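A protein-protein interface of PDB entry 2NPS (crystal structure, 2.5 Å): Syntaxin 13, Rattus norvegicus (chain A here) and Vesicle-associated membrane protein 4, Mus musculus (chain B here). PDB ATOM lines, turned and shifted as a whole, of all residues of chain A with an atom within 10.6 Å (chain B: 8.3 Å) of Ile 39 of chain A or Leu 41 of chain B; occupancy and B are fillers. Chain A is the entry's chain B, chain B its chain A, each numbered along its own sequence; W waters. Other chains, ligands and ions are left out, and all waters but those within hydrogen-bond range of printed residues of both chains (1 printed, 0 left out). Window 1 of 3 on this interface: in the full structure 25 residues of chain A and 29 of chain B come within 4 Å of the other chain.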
ATOM      1  N   ASP A  31     -14.094 -22.684 -27.263  1.00  0.00           N
ATOM      2  CA  ASP A  31     -13.384 -23.391 -26.215  1.00  0.00           C
ATOM      3  C   ASP A  31     -13.157 -22.535 -24.973  1.00  0.00           C
ATOM      4  O   ASP A  31     -13.062 -23.050 -23.863  1.00  0.00           O
ATOM      5  CB  ASP A  31     -12.050 -23.908 -26.766  1.00  0.00           C
ATOM      6  CG  ASP A  31     -12.233 -25.004 -27.813  1.00  0.00           C
ATOM      7  OD1 ASP A  31     -11.307 -25.222 -28.628  1.00  0.00           O
ATOM      8  OD2 ASP A  31     -13.305 -25.661 -27.811  1.00  0.00           O
ATOM      9  N   GLN A  32     -13.079 -21.225 -25.157  1.00  0.00           N
ATOM     10  CA  GLN A  32     -12.877 -20.306 -24.044  1.00  0.00           C
ATOM     11  C   GLN A  32     -14.115 -20.174 -23.186  1.00  0.00           C
ATOM     12  O   GLN A  32     -14.046 -19.752 -22.033  1.00  0.00           O
ATOM     13  CB  GLN A  32     -12.435 -18.945 -24.562  1.00  0.00           C
ATOM     14  CG  GLN A  32     -11.042 -19.022 -25.128  1.00  0.00           C
ATOM     15  CD  GLN A  32     -10.556 -17.741 -25.743  1.00  0.00           C
ATOM     16  OE1 GLN A  32     -11.318 -16.796 -25.958  1.00  0.00           O
ATOM     17  NE2 GLN A  32      -9.275 -17.703 -26.049  1.00  0.00           N
ATOM     18  N   GLY A  33     -15.251 -20.557 -23.749  1.00  0.00           N
ATOM     19  CA  GLY A  33     -16.494 -20.501 -23.011  1.00  0.00           C
ATOM     20  C   GLY A  33     -16.457 -21.401 -21.792  1.00  0.00           C
ATOM     21  O   GLY A  33     -17.302 -21.271 -20.911  1.00  0.00           O
ATOM     22  N   ASP A  34     -15.495 -22.321 -21.729  1.00  0.00           N
ATOM     23  CA  ASP A  34     -15.388 -23.204 -20.574  1.00  0.00           C
ATOM     24  C   ASP A  34     -14.649 -22.439 -19.482  1.00  0.00           C
ATOM     25  O   ASP A  34     -14.845 -22.683 -18.293  1.00  0.00           O
ATOM     26  CB  ASP A  34     -14.612 -24.484 -20.903  1.00  0.00           C
ATOM     27  CG  ASP A  34     -15.022 -25.105 -22.234  1.00  0.00           C
ATOM     28  OD1 ASP A  34     -16.243 -25.303 -22.469  1.00  0.00           O
ATOM     29  OD2 ASP A  34     -14.106 -25.408 -23.044  1.00  0.00           O
ATOM     30  N   LEU A  35     -13.774 -21.527 -19.888  1.00  0.00           N
ATOM     31  CA  LEU A  35     -13.077 -20.713 -18.908  1.00  0.00           C
ATOM     32  C   LEU A  35     -14.156 -19.822 -18.272  1.00  0.00           C
ATOM     33  O   LEU A  35     -14.219 -19.660 -17.057  1.00  0.00           O
ATOM     34  CB  LEU A  35     -12.004 -19.856 -19.589  1.00  0.00           C
ATOM     35  CG  LEU A  35     -10.800 -20.600 -20.175  1.00  0.00           C
ATOM     36  CD1 LEU A  35      -9.826 -19.637 -20.818  1.00  0.00           C
ATOM     37  CD2 LEU A  35     -10.104 -21.376 -19.073  1.00  0.00           C
ATOM     38  N   ILE A  36     -15.025 -19.273 -19.112  1.00  0.00           N
ATOM     39  CA  ILE A  36     -16.108 -18.422 -18.639  1.00  0.00           C
ATOM     40  C   ILE A  36     -17.040 -19.181 -17.704  1.00  0.00           C
ATOM     41  O   ILE A  36     -17.608 -18.601 -16.777  1.00  0.00           O
ATOM     42  CB  ILE A  36     -16.911 -17.851 -19.812  1.00  0.00           C
ATOM     43  CG1 ILE A  36     -16.016 -16.895 -20.601  1.00  0.00           C
ATOM     44  CG2 ILE A  36     -18.162 -17.145 -19.305  1.00  0.00           C
ATOM     45  CD1 ILE A  36     -16.526 -16.552 -21.961  1.00  0.00           C
ATOM     46  N   ASP A  37     -17.194 -20.478 -17.951  1.00  0.00           N
ATOM     47  CA  ASP A  37     -18.015 -21.339 -17.108  1.00  0.00           C
ATOM     48  C   ASP A  37     -17.416 -21.390 -15.704  1.00  0.00           C
ATOM     49  O   ASP A  37     -18.126 -21.332 -14.707  1.00  0.00           O
ATOM     50  CB  ASP A  37     -18.050 -22.762 -17.677  1.00  0.00           C
ATOM     51  CG  ASP A  37     -19.288 -23.031 -18.520  1.00  0.00           C
ATOM     52  OD1 ASP A  37     -19.128 -23.422 -19.701  1.00  0.00           O
ATOM     53  OD2 ASP A  37     -20.418 -22.859 -18.005  1.00  0.00           O
ATOM     54  N   SER A  38     -16.096 -21.492 -15.646  1.00  0.00           N
ATOM     55  CA  SER A  38     -15.374 -21.589 -14.394  1.00  0.00           C
ATOM     56  C   SER A  38     -15.435 -20.309 -13.601  1.00  0.00           C
ATOM     57  O   SER A  38     -15.727 -20.312 -12.410  1.00  0.00           O
ATOM     58  CB  SER A  38     -13.930 -21.914 -14.689  1.00  0.00           C
ATOM     59  OG  SER A  38     -13.849 -22.982 -15.598  1.00  0.00           O
ATOM     60  N   ILE A  39     -15.123 -19.223 -14.292  1.00  0.00           N
ATOM     61  CA  ILE A  39     -15.123 -17.890 -13.729  1.00  0.00           C
ATOM     62  C   ILE A  39     -16.493 -17.619 -13.139  1.00  0.00           C
ATOM     63  O   ILE A  39     -16.622 -17.242 -11.979  1.00  0.00           O
ATOM     64  CB  ILE A  39     -14.818 -16.869 -14.846  1.00  0.00           C
ATOM     65  CG1 ILE A  39     -13.383 -17.070 -15.339  1.00  0.00           C
ATOM     66  CG2 ILE A  39     -15.054 -15.458 -14.356  1.00  0.00           C
ATOM     67  CD1 ILE A  39     -13.157 -16.605 -16.741  1.00  0.00           C
ATOM     68  N   GLU A  40     -17.507 -17.829 -13.969  1.00  0.00           N
ATOM     69  CA  GLU A  40     -18.907 -17.641 -13.621  1.00  0.00           C
ATOM     70  C   GLU A  40     -19.277 -18.436 -12.384  1.00  0.00           C
ATOM     71  O   GLU A  40     -19.940 -17.925 -11.496  1.00  0.00           O
ATOM     72  CB  GLU A  40     -19.762 -18.087 -14.805  1.00  0.00           C
ATOM     73  CG  GLU A  40     -21.252 -17.876 -14.680  1.00  0.00           C
ATOM     74  CD  GLU A  40     -21.859 -17.403 -15.992  1.00  0.00           C
ATOM     75  OE1 GLU A  40     -21.650 -18.079 -17.026  1.00  0.00           O
ATOM     76  OE2 GLU A  40     -22.540 -16.346 -15.985  1.00  0.00           O
ATOM     77  N   ALA A  41     -18.852 -19.690 -12.334  1.00  0.00           N
ATOM     78  CA  ALA A  41     -19.148 -20.552 -11.203  1.00  0.00           C
ATOM     79  C   ALA A  41     -18.404 -20.102  -9.959  1.00  0.00           C
ATOM     80  O   ALA A  41     -18.947 -20.133  -8.860  1.00  0.00           O
ATOM     81  CB  ALA A  41     -18.774 -21.973 -11.536  1.00  0.00           C
ATOM     82  N   ASN A  42     -17.156 -19.690 -10.143  1.00  0.00           N
ATOM     83  CA  ASN A  42     -16.328 -19.233  -9.039  1.00  0.00           C
ATOM     84  C   ASN A  42     -16.880 -18.002  -8.349  1.00  0.00           C
ATOM     85  O   ASN A  42     -16.916 -17.932  -7.132  1.00  0.00           O
ATOM     86  CB  ASN A  42     -14.907 -18.968  -9.528  1.00  0.00           C
ATOM     87  CG  ASN A  42     -14.157 -20.243  -9.810  1.00  0.00           C
ATOM     88  OD1 ASN A  42     -14.132 -21.135  -8.977  1.00  0.00           O
ATOM     89  ND2 ASN A  42     -13.545 -20.341 -10.981  1.00  0.00           N
ATOM     90  N   VAL A  43     -17.309 -17.030  -9.140  1.00  0.00           N
ATOM     91  CA  VAL A  43     -17.893 -15.817  -8.595  1.00  0.00           C
ATOM     92  C   VAL A  43     -19.214 -16.144  -7.922  1.00  0.00           C
ATOM     93  O   VAL A  43     -19.504 -15.645  -6.845  1.00  0.00           O
ATOM     94  CB  VAL A  43     -18.126 -14.781  -9.696  1.00  0.00           C
ATOM     95  CG1 VAL A  43     -19.006 -13.665  -9.188  1.00  0.00           C
ATOM     96  CG2 VAL A  43     -16.796 -14.233 -10.157  1.00  0.00           C
ATOM     97  N   GLU A  44     -20.009 -16.991  -8.556  1.00  0.00           N
ATOM     98  CA  GLU A  44     -21.282 -17.399  -7.992  1.00  0.00           C
ATOM     99  C   GLU A  44     -21.042 -17.944  -6.608  1.00  0.00           C
ATOM    100  O   GLU A  44     -21.667 -17.523  -5.640  1.00  0.00           O
ATOM    101  CB  GLU A  44     -21.915 -18.493  -8.822  1.00  0.00           C
ATOM    102  CG  GLU A  44     -23.278 -18.861  -8.302  1.00  0.00           C
ATOM    103  CD  GLU A  44     -24.237 -17.675  -8.374  1.00  0.00           C
ATOM    104  OE1 GLU A  44     -25.263 -17.686  -7.655  1.00  0.00           O
ATOM    105  OE2 GLU A  44     -23.967 -16.730  -9.159  1.00  0.00           O
ATOM    106  N   SER A  45     -20.112 -18.885  -6.524  1.00  0.00           N
ATOM    107  CA  SER A  45     -19.750 -19.499  -5.262  1.00  0.00           C
ATOM    108  C   SER A  45     -19.297 -18.438  -4.236  1.00  0.00           C
ATOM    109  O   SER A  45     -19.700 -18.469  -3.069  1.00  0.00           O
ATOM    110  CB  SER A  45     -18.644 -20.517  -5.504  1.00  0.00           C
ATOM    111  OG  SER A  45     -18.428 -21.284  -4.346  1.00  0.00           O
ATOM    112  N   SER A  46     -18.459 -17.506  -4.663  1.00  0.00           N
ATOM    113  CA  SER A  46     -17.993 -16.450  -3.775  1.00  0.00           C
ATOM    114  C   SER A  46     -19.189 -15.641  -3.248  1.00  0.00           C
ATOM    115  O   SER A  46     -19.301 -15.368  -2.056  1.00  0.00           O
ATOM    116  CB  SER A  46     -17.029 -15.512  -4.520  1.00  0.00           C
ATOM    117  OG  SER A  46     -15.856 -16.184  -4.939  1.00  0.00           O
ATOM    118  N   GLU A  47     -20.079 -15.274  -4.160  1.00  0.00           N
ATOM    119  CA  GLU A  47     -21.272 -14.513  -3.845  1.00  0.00           C
ATOM    120  C   GLU A  47     -22.108 -15.244  -2.796  1.00  0.00           C
ATOM    121  O   GLU A  47     -22.535 -14.656  -1.792  1.00  0.00           O
ATOM    122  CB  GLU A  47     -22.082 -14.323  -5.126  1.00  0.00           C
ATOM    123  CG  GLU A  47     -23.152 -13.248  -5.077  1.00  0.00           C
ATOM    124  CD  GLU A  47     -24.209 -13.511  -4.026  1.00  0.00           C
ATOM    125  OE1 GLU A  47     -24.757 -14.637  -3.976  1.00  0.00           O
ATOM    126  OE2 GLU A  47     -24.501 -12.574  -3.251  1.00  0.00           O
ATOM    127  N   ARG B  34      -7.203 -12.988 -25.310  1.00  0.00           N
ATOM    128  CA  ARG B  34      -8.421 -13.151 -24.538  1.00  0.00           C
ATOM    129  C   ARG B  34      -8.386 -14.432 -23.705  1.00  0.00           C
ATOM    130  O   ARG B  34      -8.836 -14.448 -22.558  1.00  0.00           O
ATOM    131  CB  ARG B  34      -9.626 -13.169 -25.474  1.00  0.00           C
ATOM    132  CG  ARG B  34     -10.934 -13.032 -24.740  1.00  0.00           C
ATOM    133  CD  ARG B  34     -12.139 -12.964 -25.658  1.00  0.00           C
ATOM    134  NE  ARG B  34     -12.777 -14.261 -25.781  1.00  0.00           N
ATOM    135  CZ  ARG B  34     -14.083 -14.472 -25.661  1.00  0.00           C
ATOM    136  NH1 ARG B  34     -14.573 -15.702 -25.790  1.00  0.00           N
ATOM    137  NH2 ARG B  34     -14.895 -13.462 -25.411  1.00  0.00           N
ATOM    138  N   GLY B  35      -7.855 -15.503 -24.285  1.00  0.00           N
ATOM    139  CA  GLY B  35      -7.767 -16.760 -23.566  1.00  0.00           C
ATOM    140  C   GLY B  35      -6.886 -16.606 -22.342  1.00  0.00           C
ATOM    141  O   GLY B  35      -7.204 -17.118 -21.268  1.00  0.00           O
ATOM    142  N   GLU B  36      -5.781 -15.887 -22.503  1.00  0.00           N
ATOM    143  CA  GLU B  36      -4.839 -15.653 -21.413  1.00  0.00           C
ATOM    144  C   GLU B  36      -5.432 -14.832 -20.282  1.00  0.00           C
ATOM    145  O   GLU B  36      -5.142 -15.077 -19.106  1.00  0.00           O
ATOM    146  CB  GLU B  36      -3.591 -14.945 -21.928  1.00  0.00           C
ATOM    147  CG  GLU B  36      -2.746 -15.802 -22.826  1.00  0.00           C
ATOM    148  CD  GLU B  36      -1.375 -15.213 -23.051  1.00  0.00           C
ATOM    149  OE1 GLU B  36      -0.582 -15.799 -23.836  1.00  0.00           O
ATOM    150  OE2 GLU B  36      -1.091 -14.167 -22.431  1.00  0.00           O
ATOM    151  N   ARG B  37      -6.251 -13.850 -20.630  1.00  0.00           N
ATOM    152  CA  ARG B  37      -6.871 -13.033 -19.611  1.00  0.00           C
ATOM    153  C   ARG B  37      -7.956 -13.864 -18.937  1.00  0.00           C
ATOM    154  O   ARG B  37      -8.164 -13.773 -17.726  1.00  0.00           O
ATOM    155  CB  ARG B  37      -7.450 -11.761 -20.230  1.00  0.00           C
ATOM    156  CG  ARG B  37      -6.504 -11.055 -21.207  1.00  0.00           C
ATOM    157  CD  ARG B  37      -5.110 -10.729 -20.612  1.00  0.00           C
ATOM    158  NE  ARG B  37      -4.040 -11.532 -21.220  1.00  0.00           N
ATOM    159  CZ  ARG B  37      -2.763 -11.522 -20.833  1.00  0.00           C
ATOM    160  NH1 ARG B  37      -2.363 -10.749 -19.829  1.00  0.00           N
ATOM    161  NH2 ARG B  37      -1.881 -12.289 -21.453  1.00  0.00           N
ATOM    162  N   LEU B  38      -8.650 -14.691 -19.711  1.00  0.00           N
ATOM    163  CA  LEU B  38      -9.675 -15.535 -19.112  1.00  0.00           C
ATOM    164  C   LEU B  38      -8.996 -16.489 -18.144  1.00  0.00           C
ATOM    165  O   LEU B  38      -9.528 -16.780 -17.080  1.00  0.00           O
ATOM    166  CB  LEU B  38     -10.451 -16.299 -20.183  1.00  0.00           C
ATOM    167  CG  LEU B  38     -11.547 -15.480 -20.878  1.00  0.00           C
ATOM    168  CD1 LEU B  38     -12.116 -16.271 -22.036  1.00  0.00           C
ATOM    169  CD2 LEU B  38     -12.648 -15.132 -19.908  1.00  0.00           C
ATOM    170  N   ASP B  39      -7.802 -16.950 -18.511  1.00  0.00           N
ATOM    171  CA  ASP B  39      -7.033 -17.850 -17.665  1.00  0.00           C
ATOM    172  C   ASP B  39      -6.671 -17.203 -16.340  1.00  0.00           C
ATOM    173  O   ASP B  39      -6.743 -17.842 -15.298  1.00  0.00           O
ATOM    174  CB  ASP B  39      -5.764 -18.309 -18.387  1.00  0.00           C
ATOM    175  CG  ASP B  39      -5.866 -19.739 -18.890  1.00  0.00           C
ATOM    176  OD1 ASP B  39      -5.469 -20.007 -20.045  1.00  0.00           O
ATOM    177  OD2 ASP B  39      -6.339 -20.604 -18.126  1.00  0.00           O
ATOM    178  N   GLU B  40      -6.279 -15.936 -16.366  1.00  0.00           N
ATOM    179  CA  GLU B  40      -5.939 -15.243 -15.136  1.00  0.00           C
ATOM    180  C   GLU B  40      -7.219 -14.994 -14.328  1.00  0.00           C
ATOM    181  O   GLU B  40      -7.211 -15.064 -13.101  1.00  0.00           O
ATOM    182  CB  GLU B  40      -5.267 -13.895 -15.436  1.00  0.00           C
ATOM    183  CG  GLU B  40      -3.971 -13.930 -16.239  1.00  0.00           C
ATOM    184  CD  GLU B  40      -3.385 -12.523 -16.465  1.00  0.00           C
ATOM    185  OE1 GLU B  40      -3.054 -11.841 -15.469  1.00  0.00           O
ATOM    186  OE2 GLU B  40      -3.261 -12.090 -17.634  1.00  0.00           O
ATOM    187  N   LEU B  41      -8.312 -14.687 -15.022  1.00  0.00           N
ATOM    188  CA  LEU B  41      -9.594 -14.416 -14.375  1.00  0.00           C
ATOM    189  C   LEU B  41     -10.096 -15.638 -13.633  1.00  0.00           C
ATOM    190  O   LEU B  41     -10.665 -15.550 -12.544  1.00  0.00           O
ATOM    191  CB  LEU B  41     -10.640 -14.004 -15.418  1.00  0.00           C
ATOM    192  CG  LEU B  41     -10.992 -12.529 -15.674  1.00  0.00           C
ATOM    193  CD1 LEU B  41      -9.860 -11.604 -15.272  1.00  0.00           C
ATOM    194  CD2 LEU B  41     -11.325 -12.346 -17.146  1.00  0.00           C
ATOM    195  N   GLN B  42      -9.880 -16.792 -14.242  1.00  0.00           N
ATOM    196  CA  GLN B  42     -10.320 -18.030 -13.666  1.00  0.00           C
ATOM    197  C   GLN B  42      -9.478 -18.364 -12.439  1.00  0.00           C
ATOM    198  O   GLN B  42      -9.990 -18.851 -11.442  1.00  0.00           O
ATOM    199  CB  GLN B  42     -10.251 -19.111 -14.738  1.00  0.00           C
ATOM    200  CG  GLN B  42     -11.212 -20.251 -14.521  1.00  0.00           C
ATOM    201  CD  GLN B  42     -10.543 -21.397 -13.833  1.00  0.00           C
ATOM    202  OE1 GLN B  42      -9.672 -22.040 -14.418  1.00  0.00           O
ATOM    203  NE2 GLN B  42     -10.918 -21.654 -12.580  1.00  0.00           N
ATOM    204  N   ASP B  43      -8.189 -18.060 -12.493  1.00  0.00           N
ATOM    205  CA  ASP B  43      -7.330 -18.311 -11.351  1.00  0.00           C
ATOM    206  C   ASP B  43      -7.686 -17.403 -10.178  1.00  0.00           C
ATOM    207  O   ASP B  43      -7.744 -17.857  -9.042  1.00  0.00           O
ATOM    208  CB  ASP B  43      -5.864 -18.138 -11.737  1.00  0.00           C
ATOM    209  CG  ASP B  43      -5.324 -19.337 -12.518  1.00  0.00           C
ATOM    210  OD1 ASP B  43      -4.168 -19.763 -12.261  1.00  0.00           O
ATOM    211  OD2 ASP B  43      -6.047 -19.867 -13.395  1.00  0.00           O
ATOM    212  N   LYS B  44      -7.949 -16.125 -10.448  1.00  0.00           N
ATOM    213  CA  LYS B  44      -8.308 -15.194  -9.386  1.00  0.00           C
ATOM    214  C   LYS B  44      -9.682 -15.469  -8.803  1.00  0.00           C
ATOM    215  O   LYS B  44      -9.831 -15.468  -7.586  1.00  0.00           O
ATOM    216  CB  LYS B  44      -8.269 -13.758  -9.881  1.00  0.00           C
ATOM    217  CG  LYS B  44      -6.907 -13.247 -10.290  1.00  0.00           C
ATOM    218  CD  LYS B  44      -7.055 -11.821 -10.819  1.00  0.00           C
ATOM    219  CE  LYS B  44      -5.742 -11.212 -11.259  1.00  0.00           C
ATOM    220  NZ  LYS B  44      -5.976  -9.810 -11.689  1.00  0.00           N
ATOM    221  N   SER B  45     -10.688 -15.704  -9.645  1.00  0.00           N
ATOM    222  CA  SER B  45     -12.030 -15.977  -9.121  1.00  0.00           C
ATOM    223  C   SER B  45     -12.003 -17.282  -8.333  1.00  0.00           C
ATOM    224  O   SER B  45     -12.893 -17.587  -7.545  1.00  0.00           O
ATOM    225  CB  SER B  45     -13.061 -16.061 -10.245  1.00  0.00           C
ATOM    226  OG  SER B  45     -12.819 -17.170 -11.074  1.00  0.00           O
ATOM    227  N   GLU B  46     -10.933 -18.026  -8.540  1.00  0.00           N
ATOM    228  CA  GLU B  46     -10.687 -19.286  -7.886  1.00  0.00           C
ATOM    229  C   GLU B  46     -10.202 -19.081  -6.459  1.00  0.00           C
ATOM    230  O   GLU B  46     -10.645 -19.765  -5.542  1.00  0.00           O
ATOM    231  CB  GLU B  46      -9.627 -19.985  -8.664  1.00  0.00           C
ATOM    232  CG  GLU B  46      -9.720 -21.446  -8.705  1.00  0.00           C
ATOM    233  CD  GLU B  46      -8.533 -21.982  -9.402  1.00  0.00           C
ATOM    234  OE1 GLU B  46      -7.425 -21.880  -8.825  1.00  0.00           O
ATOM    235  OE2 GLU B  46      -8.700 -22.477 -10.532  1.00  0.00           O
ATOM    236  N   SER B  47      -9.261 -18.159  -6.276  1.00  0.00           N
ATOM    237  CA  SER B  47      -8.754 -17.845  -4.944  1.00  0.00           C
ATOM    238  C   SER B  47      -9.853 -17.174  -4.147  1.00  0.00           C
ATOM    239  O   SER B  47      -9.975 -17.373  -2.946  1.00  0.00           O
ATOM    240  CB  SER B  47      -7.571 -16.890  -5.022  1.00  0.00           C
ATOM    241  OG  SER B  47      -6.541 -17.452  -5.797  1.00  0.00           O
ATOM    242  N   LEU B  48     -10.644 -16.360  -4.831  1.00  0.00           N
ATOM    243  CA  LEU B  48     -11.741 -15.656  -4.189  1.00  0.00           C
ATOM    244  C   LEU B  48     -12.676 -16.691  -3.617  1.00  0.00           C
ATOM    245  O   LEU B  48     -13.028 -16.653  -2.441  1.00  0.00           O
ATOM    246  CB  LEU B  48     -12.478 -14.796  -5.211  1.00  0.00           C
ATOM    247  CG  LEU B  48     -13.544 -13.810  -4.724  1.00  0.00           C
ATOM    248  CD1 LEU B  48     -12.918 -12.739  -3.818  1.00  0.00           C
ATOM    249  CD2 LEU B  48     -14.208 -13.174  -5.940  1.00  0.00           C
ATOM    250  N   SER B  49     -13.055 -17.633  -4.468  1.00  0.00           N
ATOM    251  CA  SER B  49     -13.949 -18.699  -4.080  1.00  0.00           C
ATOM    252  C   SER B  49     -13.339 -19.451  -2.919  1.00  0.00           C
ATOM    253  O   SER B  49     -13.994 -19.688  -1.915  1.00  0.00           O
ATOM    254  CB  SER B  49     -14.181 -19.634  -5.254  1.00  0.00           C
ATOM    255  OG  SER B  49     -15.321 -20.417  -5.008  1.00  0.00           O
HETATM  256  O   HOH W   1     -16.426 -19.907  -2.686  1.00  0.00           O
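Hydrophobic or aromatic side chains of chain B within 4 Å of the printed part of chain A: Leu 38, Leu 41 and Leu 48. Hydrophobic or aromatic side chains of chain A within 4 Å of the printed part of chain B: Leu 35, Ile 36 and Ile 39.
Ile 39 of chain A touches just these residues of chain B: Leu 38, Leu 41, Gln 42 and Ser 45. Of chain B, only Gln 42 (3.2 Å) comes within 4 Å of Ser 38 of chain A. No residue of chain A comes within 4 Å of Glu 40 of chain B. Gln 42 of chain B touches four residues of chain A. No residue of chain A comes within 4 Å of Lys 44 of chain B. Of chain A, only Ile 39 and Asn 42 come within 4 Å of Ser 45 of chain B. Of the printed residues of chain B, Ile 36 of chain A touches Leu 38. Printed residues of chain A within 4 Å of Arg 34 of chain B: Gln 32 (2.9 Å). Printed residues of chain B within 4 Å of Ser 45 of chain A: Ser 49. Asp 34 of chain A touches none of the printed residues of chain B. The nearest residue of chain A that does not touch Leu 41 of chain B is Asn 42 of chain A (5.8 Å).
The side-chain amide nitrogen (ND2) of Asn 42 of chain A lies close to the side-chain amide nitrogen (NE2) of Gln 42 of chain B (3.3 Å). N of Ser 49 of chain B lies within hydrogen-bond range of OG of Ser 46 of chain A (3.2 Å). The side-chain hydroxyl of Ser 45 of chain B sits close to the side-chain amide nitrogen of Asn 42 of chain A (3.3 Å). The side-chain amide nitrogen of Gln 32 of chain A lies close to the backbone NH of Gly 35 of chain B (3.2 Å). OG of Ser 45 of chain A lies within hydrogen-bond range of OG of Ser 49 of chain B (3.3 Å). The guanidinium group (NE) of Arg 34 of chain B sits at hydrogen-bond distance from the side-chain amide oxygen (OE1) of Gln 32 of chain A, at 2.9 Å.
The side-chain carboxylate of Glu 46 of chain B lies within hydrogen-bond range of the side-chain amide nitrogen of Gln 42 of chain B, at 3.1 Å. The backbone carbonyl oxygen (O) of Leu 41 of chain B is in hydrogen-bond range of the side-chain hydroxyl (OG) of Ser 45 of chain B (3.1 Å). The side-chain hydroxyl (OG) of Ser 38 of chain A sits at hydrogen-bond distance from the backbone carbonyl oxygen (O) of Asp 34 of chain A, at 2.9 Å. O of Gln 42 of chain B sits at hydrogen-bond distance from OG of Ser 45 of chain B, at 3.3 Å. ND2 of Asn 42 of chain A lies within hydrogen-bond range of O of Ser 38 of chain A (2.6 Å). The side-chain hydroxyl (OG) of Ser 46 of chain A is in hydrogen-bond range of the backbone carbonyl oxygen (O) of Asn 42 of chain A, at 3.0 Å.
Water W1 bridges O of Ser 49 of chain B (2.6 Å) and OG of Ser 45 of chain A (2.9 Å).
Among the printed residues, pairs that only touch across the chains: Ser 38 of chain A with Gln 42 of chain B (3.2 Å), Ser 46 of chain A with Leu 48 of chain B (3.3 Å), Leu 35 of chain A with Leu 38 of chain B (3.5 Å), Ile 39 of chain A with Leu 38 of chain B (3.5 Å), Ile 39 of chain A with Ser 45 of chain B (3.6 Å), Ile 39 of chain A with Gln 42 of chain B (3.6 Å), Asn 42 of chain A with Ser 49 of chain B (3.6 Å), Leu 35 of chain A with Gly 35 of chain B (3.7 Å), Gln 32 of chain A with Leu 38 of chain B (3.7 Å), Ile 39 of chain A with Leu 41 of chain B (3.9 Å), Ile 36 of chain A with Leu 38 of chain B (3.9 Å), Leu 35 of chain A with Asp 39 of chain B (3.96 Å) and Leu 35 of chain A with Gln 42 of chain B (3.98 Å).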
